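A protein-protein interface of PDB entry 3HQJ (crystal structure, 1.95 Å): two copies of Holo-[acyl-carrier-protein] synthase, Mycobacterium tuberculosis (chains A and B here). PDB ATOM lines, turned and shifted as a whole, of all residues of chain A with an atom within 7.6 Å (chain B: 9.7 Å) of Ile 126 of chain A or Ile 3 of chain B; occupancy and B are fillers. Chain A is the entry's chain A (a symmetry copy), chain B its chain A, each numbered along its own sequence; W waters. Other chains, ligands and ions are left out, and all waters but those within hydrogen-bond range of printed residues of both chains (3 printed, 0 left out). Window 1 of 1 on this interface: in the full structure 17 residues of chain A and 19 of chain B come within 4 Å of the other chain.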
ATOM      1  N   GLY A   2     -28.317  -1.572 -15.544  1.00  0.00           N
ATOM      2  CA  GLY A   2     -27.308  -2.576 -15.117  1.00  0.00           C
ATOM      3  C   GLY A   2     -25.876  -2.115 -15.354  1.00  0.00           C
ATOM      4  O   GLY A   2     -25.615  -0.975 -15.718  1.00  0.00           O
ATOM      5  N   ILE A   3     -24.943  -3.035 -15.177  1.00  0.00           N
ATOM      6  CA  ILE A   3     -23.541  -2.719 -15.320  1.00  0.00           C
ATOM      7  C   ILE A   3     -23.151  -2.640 -16.806  1.00  0.00           C
ATOM      8  O   ILE A   3     -23.539  -3.491 -17.630  1.00  0.00           O
ATOM      9  CB  ILE A   3     -22.687  -3.763 -14.533  1.00  0.00           C
ATOM     10  CG1 ILE A   3     -22.944  -3.593 -13.027  1.00  0.00           C
ATOM     11  CG2 ILE A   3     -21.180  -3.603 -14.869  1.00  0.00           C
ATOM     12  CD1 ILE A   3     -22.555  -4.820 -12.149  1.00  0.00           C
ATOM     13  N   VAL A   4     -22.418  -1.592 -17.147  1.00  0.00           N
ATOM     14  CA  VAL A   4     -21.838  -1.433 -18.484  1.00  0.00           C
ATOM     15  C   VAL A   4     -20.525  -2.197 -18.660  1.00  0.00           C
ATOM     16  O   VAL A   4     -20.311  -2.907 -19.656  1.00  0.00           O
ATOM     17  CB  VAL A   4     -21.638   0.079 -18.778  1.00  0.00           C
ATOM     18  CG1 VAL A   4     -20.802   0.320 -20.024  1.00  0.00           C
ATOM     19  CG2 VAL A   4     -23.018   0.764 -18.893  1.00  0.00           C
ATOM     20  N   GLY A   5     -19.642  -2.037 -17.676  1.00  0.00           N
ATOM     21  CA  GLY A   5     -18.348  -2.683 -17.694  1.00  0.00           C
ATOM     22  C   GLY A   5     -17.635  -2.459 -16.377  1.00  0.00           C
ATOM     23  O   GLY A   5     -18.123  -1.725 -15.483  1.00  0.00           O
ATOM     24  N   VAL A   6     -16.507  -3.150 -16.265  1.00  0.00           N
ATOM     25  CA  VAL A   6     -15.586  -3.049 -15.113  1.00  0.00           C
ATOM     26  C   VAL A   6     -14.163  -2.964 -15.675  1.00  0.00           C
ATOM     27  O   VAL A   6     -13.890  -3.484 -16.732  1.00  0.00           O
ATOM     28  CB  VAL A   6     -15.748  -4.241 -14.099  1.00  0.00           C
ATOM     29  CG1 VAL A   6     -15.363  -5.613 -14.718  1.00  0.00           C
ATOM     30  CG2 VAL A   6     -14.944  -3.999 -12.784  1.00  0.00           C
ATOM     31  N   GLY A   7     -13.279  -2.256 -14.982  1.00  0.00           N
ATOM     32  CA  GLY A   7     -11.891  -2.254 -15.369  1.00  0.00           C
ATOM     33  C   GLY A   7     -11.037  -2.291 -14.132  1.00  0.00           C
ATOM     34  O   GLY A   7     -11.435  -1.834 -13.048  1.00  0.00           O
ATOM     35  N   ALA A  59      -8.654   2.186 -15.839  1.00  0.00           N
ATOM     36  CA  ALA A  59      -9.750   1.313 -15.414  1.00  0.00           C
ATOM     37  C   ALA A  59     -11.038   1.771 -16.071  1.00  0.00           C
ATOM     38  O   ALA A  59     -11.807   0.951 -16.519  1.00  0.00           O
ATOM     39  CB  ALA A  59      -9.901   1.332 -13.887  1.00  0.00           C
ATOM     40  N   VAL A  60     -11.259   3.088 -16.117  1.00  0.00           N
ATOM     41  CA  VAL A  60     -12.488   3.646 -16.724  1.00  0.00           C
ATOM     42  C   VAL A  60     -12.536   3.308 -18.208  1.00  0.00           C
ATOM     43  O   VAL A  60     -13.575   2.868 -18.732  1.00  0.00           O
ATOM     44  CB  VAL A  60     -12.591   5.181 -16.509  1.00  0.00           C
ATOM     45  CG1 VAL A  60     -13.736   5.770 -17.385  1.00  0.00           C
ATOM     46  CG2 VAL A  60     -12.846   5.498 -15.021  1.00  0.00           C
ATOM     47  N   ALA A  63     -13.311  -0.374 -18.660  1.00  0.00           N
ATOM     48  CA  ALA A  63     -14.730  -0.635 -18.373  1.00  0.00           C
ATOM     49  C   ALA A  63     -15.620  -0.210 -19.552  1.00  0.00           C
ATOM     50  O   ALA A  63     -16.564  -0.919 -19.923  1.00  0.00           O
ATOM     51  CB  ALA A  63     -15.122   0.127 -17.110  1.00  0.00           C
ATOM     52  N   TRP A  64     -15.338   0.954 -20.121  1.00  0.00           N
ATOM     53  CA  TRP A  64     -16.174   1.435 -21.226  1.00  0.00           C
ATOM     54  C   TRP A  64     -15.906   0.645 -22.504  1.00  0.00           C
ATOM     55  O   TRP A  64     -16.832   0.094 -23.087  1.00  0.00           O
ATOM     56  CB  TRP A  64     -16.030   2.931 -21.515  1.00  0.00           C
ATOM     57  CG  TRP A  64     -17.019   3.338 -22.656  1.00  0.00           C
ATOM     58  CD1 TRP A  64     -18.383   3.163 -22.663  1.00  0.00           C
ATOM     59  CD2 TRP A  64     -16.685   3.910 -23.919  1.00  0.00           C
ATOM     60  NE1 TRP A  64     -18.916   3.616 -23.853  1.00  0.00           N
ATOM     61  CE2 TRP A  64     -17.893   4.073 -24.643  1.00  0.00           C
ATOM     62  CE3 TRP A  64     -15.483   4.320 -24.508  1.00  0.00           C
ATOM     63  CZ2 TRP A  64     -17.932   4.628 -25.920  1.00  0.00           C
ATOM     64  CZ3 TRP A  64     -15.519   4.867 -25.781  1.00  0.00           C
ATOM     65  CH2 TRP A  64     -16.740   5.017 -26.477  1.00  0.00           C
ATOM     66  N   VAL A 108     -24.193   7.515 -18.072  1.00  0.00           N
ATOM     67  CA  VAL A 108     -23.459   6.489 -17.317  1.00  0.00           C
ATOM     68  C   VAL A 108     -22.900   7.022 -15.976  1.00  0.00           C
ATOM     69  O   VAL A 108     -22.268   8.077 -15.924  1.00  0.00           O
ATOM     70  CB  VAL A 108     -22.338   5.861 -18.212  1.00  0.00           C
ATOM     71  CG1 VAL A 108     -21.466   4.864 -17.444  1.00  0.00           C
ATOM     72  CG2 VAL A 108     -22.945   5.152 -19.443  1.00  0.00           C
ATOM     73  N   THR A 109     -23.149   6.284 -14.899  1.00  0.00           N
ATOM     74  CA  THR A 109     -22.601   6.599 -13.569  1.00  0.00           C
ATOM     75  C   THR A 109     -21.270   5.842 -13.429  1.00  0.00           C
ATOM     76  O   THR A 109     -21.177   4.670 -13.775  1.00  0.00           O
ATOM     77  CB  THR A 109     -23.595   6.174 -12.484  1.00  0.00           C
ATOM     78  OG1 THR A 109     -24.795   6.939 -12.651  1.00  0.00           O
ATOM     79  CG2 THR A 109     -23.045   6.395 -11.041  1.00  0.00           C
ATOM     80  N   ILE A 110     -20.235   6.530 -12.991  1.00  0.00           N
ATOM     81  CA  ILE A 110     -18.920   5.890 -12.828  1.00  0.00           C
ATOM     82  C   ILE A 110     -18.591   5.779 -11.345  1.00  0.00           C
ATOM     83  O   ILE A 110     -18.640   6.780 -10.610  1.00  0.00           O
ATOM     84  CB  ILE A 110     -17.832   6.699 -13.540  1.00  0.00           C
ATOM     85  CG1 ILE A 110     -18.084   6.717 -15.041  1.00  0.00           C
ATOM     86  CG2 ILE A 110     -16.397   6.158 -13.221  1.00  0.00           C
ATOM     87  CD1 ILE A 110     -17.064   7.563 -15.785  1.00  0.00           C
ATOM     88  N   HIS A 111     -18.231   4.566 -10.916  1.00  0.00           N
ATOM     89  CA  HIS A 111     -17.762   4.335  -9.555  1.00  0.00           C
ATOM     90  C   HIS A 111     -16.286   3.944  -9.641  1.00  0.00           C
ATOM     91  O   HIS A 111     -15.920   3.141 -10.487  1.00  0.00           O
ATOM     92  CB  HIS A 111     -18.557   3.201  -8.907  1.00  0.00           C
ATOM     93  CG  HIS A 111     -20.039   3.462  -8.844  1.00  0.00           C
ATOM     94  ND1 HIS A 111     -20.929   2.971  -9.777  1.00  0.00           N
ATOM     95  CD2 HIS A 111     -20.778   4.148  -7.948  1.00  0.00           C
ATOM     96  CE1 HIS A 111     -22.154   3.356  -9.466  1.00  0.00           C
ATOM     97  NE2 HIS A 111     -22.092   4.075  -8.360  1.00  0.00           N
ATOM     98  N   VAL A 112     -15.445   4.557  -8.825  1.00  0.00           N
ATOM     99  CA  VAL A 112     -14.012   4.250  -8.858  1.00  0.00           C
ATOM    100  C   VAL A 112     -13.453   4.073  -7.452  1.00  0.00           C
ATOM    101  O   VAL A 112     -14.034   4.550  -6.482  1.00  0.00           O
ATOM    102  CB  VAL A 112     -13.122   5.315  -9.620  1.00  0.00           C
ATOM    103  CG1 VAL A 112     -13.466   5.375 -11.131  1.00  0.00           C
ATOM    104  CG2 VAL A 112     -13.089   6.717  -8.878  1.00  0.00           C
ATOM    105  N   SER A 113     -12.307   3.406  -7.356  1.00  0.00           N
ATOM    106  CA  SER A 113     -11.564   3.349  -6.104  1.00  0.00           C
ATOM    107  C   SER A 113     -10.091   3.250  -6.443  1.00  0.00           C
ATOM    108  O   SER A 113      -9.721   2.635  -7.462  1.00  0.00           O
ATOM    109  CB  SER A 113     -12.013   2.165  -5.239  1.00  0.00           C
ATOM    110  OG  SER A 113     -11.285   2.162  -4.000  1.00  0.00           O
ATOM    111  N   VAL A 124      -9.851   0.441  -9.595  1.00  0.00           N
ATOM    112  CA  VAL A 124     -10.945  -0.336 -10.188  1.00  0.00           C
ATOM    113  C   VAL A 124     -12.020   0.695 -10.553  1.00  0.00           C
ATOM    114  O   VAL A 124     -12.187   1.715  -9.833  1.00  0.00           O
ATOM    115  CB  VAL A 124     -11.485  -1.433  -9.192  1.00  0.00           C
ATOM    116  CG1 VAL A 124     -12.026  -0.820  -7.860  1.00  0.00           C
ATOM    117  CG2 VAL A 124     -12.585  -2.315  -9.801  1.00  0.00           C
ATOM    118  N   ALA A 125     -12.747   0.434 -11.645  1.00  0.00           N
ATOM    119  CA  ALA A 125     -13.867   1.292 -12.036  1.00  0.00           C
ATOM    120  C   ALA A 125     -15.005   0.399 -12.438  1.00  0.00           C
ATOM    121  O   ALA A 125     -14.791  -0.676 -13.049  1.00  0.00           O
ATOM    122  CB  ALA A 125     -13.485   2.197 -13.227  1.00  0.00           C
ATOM    123  N   ILE A 126     -16.220   0.840 -12.112  1.00  0.00           N
ATOM    124  CA  ILE A 126     -17.430   0.150 -12.581  1.00  0.00           C
ATOM    125  C   ILE A 126     -18.337   1.222 -13.198  1.00  0.00           C
ATOM    126  O   ILE A 126     -18.579   2.263 -12.571  1.00  0.00           O
ATOM    127  CB  ILE A 126     -18.226  -0.527 -11.423  1.00  0.00           C
ATOM    128  CG1 ILE A 126     -17.334  -1.453 -10.598  1.00  0.00           C
ATOM    129  CG2 ILE A 126     -19.515  -1.238 -11.986  1.00  0.00           C
ATOM    130  CD1 ILE A 126     -18.024  -1.958  -9.335  1.00  0.00           C
ATOM    131  N   LEU A 127     -18.759   0.988 -14.441  1.00  0.00           N
ATOM    132  CA  LEU A 127     -19.692   1.865 -15.147  1.00  0.00           C
ATOM    133  C   LEU A 127     -21.070   1.233 -15.112  1.00  0.00           C
ATOM    134  O   LEU A 127     -21.229   0.014 -15.283  1.00  0.00           O
ATOM    135  CB  LEU A 127     -19.227   2.107 -16.587  1.00  0.00           C
ATOM    136  CG  LEU A 127     -18.181   3.197 -16.814  1.00  0.00           C
ATOM    137  CD1 LEU A 127     -16.991   3.065 -15.843  1.00  0.00           C
ATOM    138  CD2 LEU A 127     -17.711   3.135 -18.253  1.00  0.00           C
ATOM    139  N   GLU A 128     -22.038   2.060 -14.842  1.00  0.00           N
ATOM    140  CA  GLU A 128     -23.376   1.630 -14.625  1.00  0.00           C
ATOM    141  C   GLU A 128     -24.362   2.551 -15.385  1.00  0.00           C
ATOM    142  O   GLU A 128     -24.249   3.717 -15.320  1.00  0.00           O
ATOM    143  CB  GLU A 128     -23.597   1.636 -13.132  1.00  0.00           C
ATOM    144  CG  GLU A 128     -24.932   1.576 -12.667  1.00  0.00           C
ATOM    145  CD  GLU A 128     -25.036   1.767 -11.194  1.00  0.00           C
ATOM    146  OE1 GLU A 128     -24.556   2.739 -10.670  1.00  0.00           O
ATOM    147  OE2 GLU A 128     -25.605   0.920 -10.590  1.00  0.00           O
ATOM    148  N   ALA A 129     -25.302   1.988 -16.104  1.00  0.00           N
ATOM    149  CA  ALA A 129     -26.209   2.791 -16.913  1.00  0.00           C
ATOM    150  C   ALA A 129     -27.645   2.536 -16.619  1.00  0.00           C
ATOM    151  O   ALA A 129     -27.951   1.936 -15.629  1.00  0.00           O
ATOM    152  CB  ALA A 129     -25.951   2.585 -18.329  1.00  0.00           C
ATOM    153  N   GLY B   2     -29.305   0.293  -7.347  1.00  0.00           N
ATOM    154  CA  GLY B   2     -28.017   0.379  -8.083  1.00  0.00           C
ATOM    155  C   GLY B   2     -26.804   0.325  -7.164  1.00  0.00           C
ATOM    156  O   GLY B   2     -26.910   0.084  -5.967  1.00  0.00           O
ATOM    157  N   ILE B   3     -25.642   0.591  -7.734  1.00  0.00           N
ATOM    158  CA  ILE B   3     -24.407   0.526  -6.989  1.00  0.00           C
ATOM    159  C   ILE B   3     -24.237   1.777  -6.109  1.00  0.00           C
ATOM    160  O   ILE B   3     -24.476   2.920  -6.544  1.00  0.00           O
ATOM    161  CB  ILE B   3     -23.212   0.322  -7.973  1.00  0.00           C
ATOM    162  CG1 ILE B   3     -23.320  -1.071  -8.615  1.00  0.00           C
ATOM    163  CG2 ILE B   3     -21.857   0.498  -7.234  1.00  0.00           C
ATOM    164  CD1 ILE B   3     -22.508  -1.254  -9.932  1.00  0.00           C
ATOM    165  N   VAL B   4     -23.864   1.547  -4.859  1.00  0.00           N
ATOM    166  CA  VAL B   4     -23.517   2.623  -3.927  1.00  0.00           C
ATOM    167  C   VAL B   4     -22.077   3.113  -4.089  1.00  0.00           C
ATOM    168  O   VAL B   4     -21.801   4.322  -4.148  1.00  0.00           O
ATOM    169  CB  VAL B   4     -23.773   2.143  -2.473  1.00  0.00           C
ATOM    170  CG1 VAL B   4     -23.193   3.093  -1.439  1.00  0.00           C
ATOM    171  CG2 VAL B   4     -25.290   1.948  -2.259  1.00  0.00           C
ATOM    172  N   GLY B   5     -21.158   2.152  -4.156  1.00  0.00           N
ATOM    173  CA  GLY B   5     -19.750   2.446  -4.301  1.00  0.00           C
ATOM    174  C   GLY B   5     -18.969   1.168  -4.522  1.00  0.00           C
ATOM    175  O   GLY B   5     -19.526   0.043  -4.477  1.00  0.00           O
ATOM    176  N   VAL B   6     -17.690   1.374  -4.814  1.00  0.00           N
ATOM    177  CA  VAL B   6     -16.698   0.293  -4.998  1.00  0.00           C
ATOM    178  C   VAL B   6     -15.432   0.706  -4.241  1.00  0.00           C
ATOM    179  O   VAL B   6     -15.159   1.875  -4.096  1.00  0.00           O
ATOM    180  CB  VAL B   6     -16.406  -0.011  -6.513  1.00  0.00           C
ATOM    181  CG1 VAL B   6     -15.740   1.185  -7.249  1.00  0.00           C
ATOM    182  CG2 VAL B   6     -15.543  -1.299  -6.691  1.00  0.00           C
ATOM    183  N   GLY B   7     -14.697  -0.266  -3.715  1.00  0.00           N
ATOM    184  CA  GLY B   7     -13.419   0.034  -3.120  1.00  0.00           C
ATOM    185  C   GLY B   7     -12.443  -1.053  -3.478  1.00  0.00           C
ATOM    186  O   GLY B   7     -12.816  -2.211  -3.726  1.00  0.00           O
ATOM    187  N   ILE B   8     -11.181  -0.685  -3.458  1.00  0.00           N
ATOM    188  CA  ILE B   8     -10.100  -1.639  -3.674  1.00  0.00           C
ATOM    189  C   ILE B   8      -9.014  -1.282  -2.672  1.00  0.00           C
ATOM    190  O   ILE B   8      -8.895  -0.122  -2.255  1.00  0.00           O
ATOM    191  CB  ILE B   8      -9.560  -1.533  -5.142  1.00  0.00           C
ATOM    192  CG1 ILE B   8      -8.624  -2.713  -5.493  1.00  0.00           C
ATOM    193  CG2 ILE B   8      -8.898  -0.162  -5.408  1.00  0.00           C
ATOM    194  CD1 ILE B   8      -8.424  -2.906  -7.016  1.00  0.00           C
ATOM    195  N   ALA B  63     -15.687   2.037  -0.432  1.00  0.00           N
ATOM    196  CA  ALA B  63     -16.936   1.952  -1.206  1.00  0.00           C
ATOM    197  C   ALA B  63     -18.045   2.799  -0.563  1.00  0.00           C
ATOM    198  O   ALA B  63     -18.797   3.493  -1.258  1.00  0.00           O
ATOM    199  CB  ALA B  63     -17.363   0.488  -1.281  1.00  0.00           C
ATOM    200  N   TRP B  64     -18.161   2.726   0.757  1.00  0.00           N
ATOM    201  CA  TRP B  64     -19.225   3.481   1.427  1.00  0.00           C
ATOM    202  C   TRP B  64     -18.909   4.974   1.450  1.00  0.00           C
ATOM    203  O   TRP B  64     -19.714   5.775   0.991  1.00  0.00           O
ATOM    204  CB  TRP B  64     -19.529   3.005   2.849  1.00  0.00           C
ATOM    205  CG  TRP B  64     -20.723   3.831   3.430  1.00  0.00           C
ATOM    206  CD1 TRP B  64     -21.978   3.958   2.883  1.00  0.00           C
ATOM    207  CD2 TRP B  64     -20.714   4.649   4.599  1.00  0.00           C
ATOM    208  NE1 TRP B  64     -22.755   4.793   3.660  1.00  0.00           N
ATOM    209  CE2 TRP B  64     -21.999   5.236   4.715  1.00  0.00           C
ATOM    210  CE3 TRP B  64     -19.749   4.933   5.573  1.00  0.00           C
ATOM    211  CZ2 TRP B  64     -22.343   6.083   5.765  1.00  0.00           C
ATOM    212  CZ3 TRP B  64     -20.088   5.783   6.615  1.00  0.00           C
ATOM    213  CH2 TRP B  64     -21.378   6.350   6.704  1.00  0.00           C
ATOM    214  N   GLY B  66     -16.809   6.631  -0.239  1.00  0.00           N
ATOM    215  CA  GLY B  66     -16.831   7.086  -1.623  1.00  0.00           C
ATOM    216  C   GLY B  66     -18.204   7.555  -2.100  1.00  0.00           C
ATOM    217  O   GLY B  66     -18.293   8.482  -2.920  1.00  0.00           O
ATOM    218  N   SER B  67     -19.275   6.926  -1.607  1.00  0.00           N
ATOM    219  CA  SER B  67     -20.646   7.363  -1.943  1.00  0.00           C
ATOM    220  C   SER B  67     -21.085   8.682  -1.253  1.00  0.00           C
ATOM    221  O   SER B  67     -22.189   9.182  -1.505  1.00  0.00           O
ATOM    222  CB  SER B  67     -21.671   6.275  -1.617  1.00  0.00           C
ATOM    223  OG  SER B  67     -21.922   6.161  -0.219  1.00  0.00           O
ATOM    224  N   VAL B 108     -28.149  -2.010   2.619  1.00  0.00           N
ATOM    225  CA  VAL B 108     -27.077  -2.193   1.629  1.00  0.00           C
ATOM    226  C   VAL B 108     -26.525  -3.639   1.608  1.00  0.00           C
ATOM    227  O   VAL B 108     -26.203  -4.212   2.648  1.00  0.00           O
ATOM    228  CB  VAL B 108     -25.945  -1.136   1.861  1.00  0.00           C
ATOM    229  CG1 VAL B 108     -24.748  -1.347   0.929  1.00  0.00           C
ATOM    230  CG2 VAL B 108     -26.482   0.300   1.670  1.00  0.00           C
ATOM    231  N   THR B 109     -26.431  -4.216   0.415  1.00  0.00           N
ATOM    232  CA  THR B 109     -25.831  -5.546   0.214  1.00  0.00           C
ATOM    233  C   THR B 109     -24.338  -5.337  -0.086  1.00  0.00           C
ATOM    234  O   THR B 109     -23.972  -4.469  -0.870  1.00  0.00           O
ATOM    235  CB  THR B 109     -26.532  -6.262  -0.944  1.00  0.00           C
ATOM    236  OG1 THR B 109     -27.906  -6.454  -0.586  1.00  0.00           O
ATOM    237  CG2 THR B 109     -25.892  -7.645  -1.275  1.00  0.00           C
ATOM    238  N   HIS B 111     -20.783  -6.996  -1.425  1.00  0.00           N
ATOM    239  CA  HIS B 111     -20.107  -8.087  -2.118  1.00  0.00           C
ATOM    240  C   HIS B 111     -18.603  -7.861  -1.964  1.00  0.00           C
ATOM    241  O   HIS B 111     -18.138  -6.742  -2.125  1.00  0.00           O
ATOM    242  CB  HIS B 111     -20.479  -8.082  -3.600  1.00  0.00           C
ATOM    243  CG  HIS B 111     -21.957  -8.225  -3.853  1.00  0.00           C
ATOM    244  ND1 HIS B 111     -22.787  -7.147  -4.088  1.00  0.00           N
ATOM    245  CD2 HIS B 111     -22.740  -9.321  -3.923  1.00  0.00           C
ATOM    246  CE1 HIS B 111     -24.023  -7.573  -4.277  1.00  0.00           C
ATOM    247  NE2 HIS B 111     -24.024  -8.890  -4.180  1.00  0.00           N
ATOM    248  N   VAL B 124     -11.502  -6.374  -2.987  1.00  0.00           N
ATOM    249  CA  VAL B 124     -12.407  -5.450  -3.679  1.00  0.00           C
ATOM    250  C   VAL B 124     -13.758  -5.602  -2.969  1.00  0.00           C
ATOM    251  O   VAL B 124     -14.108  -6.722  -2.509  1.00  0.00           O
ATOM    252  CB  VAL B 124     -12.503  -5.775  -5.220  1.00  0.00           C
ATOM    253  CG1 VAL B 124     -13.023  -7.222  -5.496  1.00  0.00           C
ATOM    254  CG2 VAL B 124     -13.387  -4.786  -5.993  1.00  0.00           C
ATOM    255  N   ALA B 125     -14.514  -4.502  -2.890  1.00  0.00           N
ATOM    256  CA  ALA B 125     -15.864  -4.546  -2.325  1.00  0.00           C
ATOM    257  C   ALA B 125     -16.756  -3.731  -3.216  1.00  0.00           C
ATOM    258  O   ALA B 125     -16.334  -2.682  -3.759  1.00  0.00           O
ATOM    259  CB  ALA B 125     -15.891  -3.954  -0.899  1.00  0.00           C
ATOM    260  N   ILE B 126     -17.996  -4.198  -3.364  1.00  0.00           N
ATOM    261  CA  ILE B 126     -19.021  -3.421  -4.076  1.00  0.00           C
ATOM    262  C   ILE B 126     -20.253  -3.378  -3.164  1.00  0.00           C
ATOM    263  O   ILE B 126     -20.691  -4.423  -2.665  1.00  0.00           O
ATOM    264  CB  ILE B 126     -19.455  -4.085  -5.419  1.00  0.00           C
ATOM    265  CG1 ILE B 126     -18.252  -4.380  -6.311  1.00  0.00           C
ATOM    266  CG2 ILE B 126     -20.561  -3.213  -6.128  1.00  0.00           C
ATOM    267  CD1 ILE B 126     -18.619  -5.222  -7.530  1.00  0.00           C
ATOM    268  N   LEU B 127     -20.744  -2.166  -2.900  1.00  0.00           N
ATOM    269  CA  LEU B 127     -21.959  -1.948  -2.116  1.00  0.00           C
ATOM    270  C   LEU B 127     -23.098  -1.637  -3.067  1.00  0.00           C
ATOM    271  O   LEU B 127     -22.940  -0.892  -4.047  1.00  0.00           O
ATOM    272  CB  LEU B 127     -21.756  -0.820  -1.100  1.00  0.00           C
ATOM    273  CG  LEU B 127     -21.082  -1.178   0.223  1.00  0.00           C
ATOM    274  CD1 LEU B 127     -19.792  -1.994   0.011  1.00  0.00           C
ATOM    275  CD2 LEU B 127     -20.792   0.098   0.987  1.00  0.00           C
ATOM    276  N   GLU B 128     -24.214  -2.248  -2.794  1.00  0.00           N
ATOM    277  CA  GLU B 128     -25.348  -2.193  -3.651  1.00  0.00           C
ATOM    278  C   GLU B 128     -26.633  -1.949  -2.821  1.00  0.00           C
ATOM    279  O   GLU B 128     -26.833  -2.574  -1.848  1.00  0.00           O
ATOM    280  CB  GLU B 128     -25.379  -3.496  -4.413  1.00  0.00           C
ATOM    281  CG  GLU B 128     -26.580  -3.838  -5.078  1.00  0.00           C
ATOM    282  CD  GLU B 128     -26.552  -5.215  -5.641  1.00  0.00           C
ATOM    283  OE1 GLU B 128     -26.295  -6.157  -4.938  1.00  0.00           O
ATOM    284  OE2 GLU B 128     -26.791  -5.318  -6.799  1.00  0.00           O
ATOM    285  N   ALA B 129     -27.464  -1.023  -3.230  1.00  0.00           N
ATOM    286  CA  ALA B 129     -28.646  -0.681  -2.452  1.00  0.00           C
ATOM    287  C   ALA B 129     -29.912  -0.776  -3.228  1.00  0.00           C
ATOM    288  O   ALA B 129     -29.921  -1.343  -4.282  1.00  0.00           O
ATOM    289  CB  ALA B 129     -28.517   0.650  -1.880  1.00  0.00           C
ATOM    290  N   PRO B 130     -31.002  -0.244  -2.667  1.00  0.00           N
ATOM    291  CA  PRO B 130     -32.326  -0.339  -3.298  1.00  0.00           C
ATOM    292  C   PRO B 130     -32.896   0.969  -3.869  1.00  0.00           C
ATOM    293  O   PRO B 130     -32.296   2.039  -3.804  1.00  0.00           O
ATOM    294  CB  PRO B 130     -33.194  -0.832  -2.141  1.00  0.00           C
ATOM    295  CG  PRO B 130     -32.265  -1.510  -1.243  1.00  0.00           C
ATOM    296  CD  PRO B 130     -31.086  -0.661  -1.254  1.00  0.00           C
HETATM  297  O   HOH W   1     -14.512   4.776  -3.601  1.00  0.00           O
HETATM  298  O   HOH W   2     -25.775   3.993  -8.592  1.00  0.00           O
HETATM  299  O   HOH W   3     -17.117   4.249  -5.641  1.00  0.00           O
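His 111 of chain A touches Ile 3 of chain B, but with the chains exchanged Ile 3 of chain A does not touch His 111 of chain B (8.4 Å). His 111 of chain A touches Val 6 of chain B, but with the chains exchanged Val 6 of chain A does not touch His 111 of chain B (11.5 Å). Val 124 of chain A touches Val 6 of chain B, but with the chains exchanged Val 6 of chain A does not touch Val 124 of chain B (7.0 Å). Of the 15 pairs that touch across the chains among the printed residues, 2 have their exchanged pair printed and touching as well.
Of the printed residues of chain B, His 111 of chain A touches Ile 3, Val 4 and Val 6. No residue of chain B comes within 4 Å of Ala 125 of chain A. No residue of chain B comes within 4 Å of Leu 127 of chain A. Of the printed residues of chain A, Gly 2 of chain B touches Glu 128. Printed residues of chain A within 4 Å of Ile 8 of chain B: Ser 113 (2.9 Å) and Val 124 (3.7 Å). Val 60 of chain A touches none of the printed residues of chain B. Thr 109 of chain A touches none of the printed residues of chain B. The nearest printed residue of chain B that does not touch Ile 3 of chain A is Ile 126 of chain B (6.1 Å).
Of the 22 printed residues of chain A, 7 touch a printed residue of chain B. Printed residues of chain A that touch a printed residue of chain B: Ile 3, His 111, Val 112, Ser 113, Val 124, Ile 126 and Glu 128. Hydrophobic or aromatic side chains of chain A within 4 Å of the printed part of chain B: Ile 3, His 111, Val 124 and Ile 126. Of the 21 printed residues of chain B, 7 touch a printed residue of chain A. Printed residues of chain B that touch a printed residue of chain A: Gly 2, Ile 3, Val 4, Val 6, Gly 7, Ile 8 and Ile 126. Hydrophobic or aromatic side chains of chain B that line the printed part of chain A: Ile 3, Val 6, Ile 8 and Ile 126. Among the printed residues, no Asp or Glu carboxylate lies within 4 Å of a Lys or Arg side-chain nitrogen of the other chain.
The backbone carbonyl oxygen (O) of Ile 3 of chain B is in hydrogen-bond range of a ring nitrogen (NE2) of His 111 of chain A, 3.2 Å away. OE2 of Glu 128 of chain A lies within hydrogen-bond range of N of Ile 3 of chain B (2.9 Å). N of Ile 8 of chain B sits at hydrogen-bond distance from OG of Ser 113 of chain A, 2.9 Å away.
Water W2 lies within hydrogen-bond range of O of Ile 3 of chain B (2.7 Å) and OE1 of Glu 128 of chain A (2.7 Å). Water W1 bridges the backbone carbonyl oxygen of Val 112 of chain A (2.9 Å) and the backbone carbonyl oxygen of Val 6 of chain B (3.0 Å). Water W3 bridges the backbone NH (N) of Val 6 of chain B (3.0 Å) and the backbone carbonyl oxygen (O) of Val 112 of chain A (3.2 Å).
The backbone NH (N) of Ala 129 of chain B lies within hydrogen-bond range of the backbone carbonyl oxygen (O) of Gly 2 of chain B, 3.0 Å away. The backbone NH (N) of Val 4 of chain B is in hydrogen-bond range of the backbone carbonyl oxygen (O) of Leu 127 of chain B. The backbone NH of Gly 7 of chain B sits at hydrogen-bond distance from the backbone carbonyl oxygen of Ala 125 of chain B. The backbone NH of Ile 126 of chain B sits at hydrogen-bond distance from the backbone carbonyl oxygen of His 111 of chain B (2.8 Å).
Ile 3 of chain A touches Ile 3 of chain B. His 111 of chain A touches Val 4 of chain B (CD2 to O, 3.9 Å). His 111 of chain A touches Val 6 of chain B (C to CG1, 3.7 Å). Val 6 of chain B touches Val 112 of chain A (CG1 to C, 3.7 Å). O of Val 6 of chain B touches CB of Ser 113 of chain A (3.4 Å). Ser 113 of chain A touches Gly 7 of chain B (OG to CA, 3.1 Å). Val 6 of chain B touches Val 124 of chain A (CG2 to CG1, 3.7 Å). CD1 of Ile 126 of chain A touches CG2 of Val 6 of chain B, at 3.7 Å. Gly 2 of chain B touches Glu 128 of chain A.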
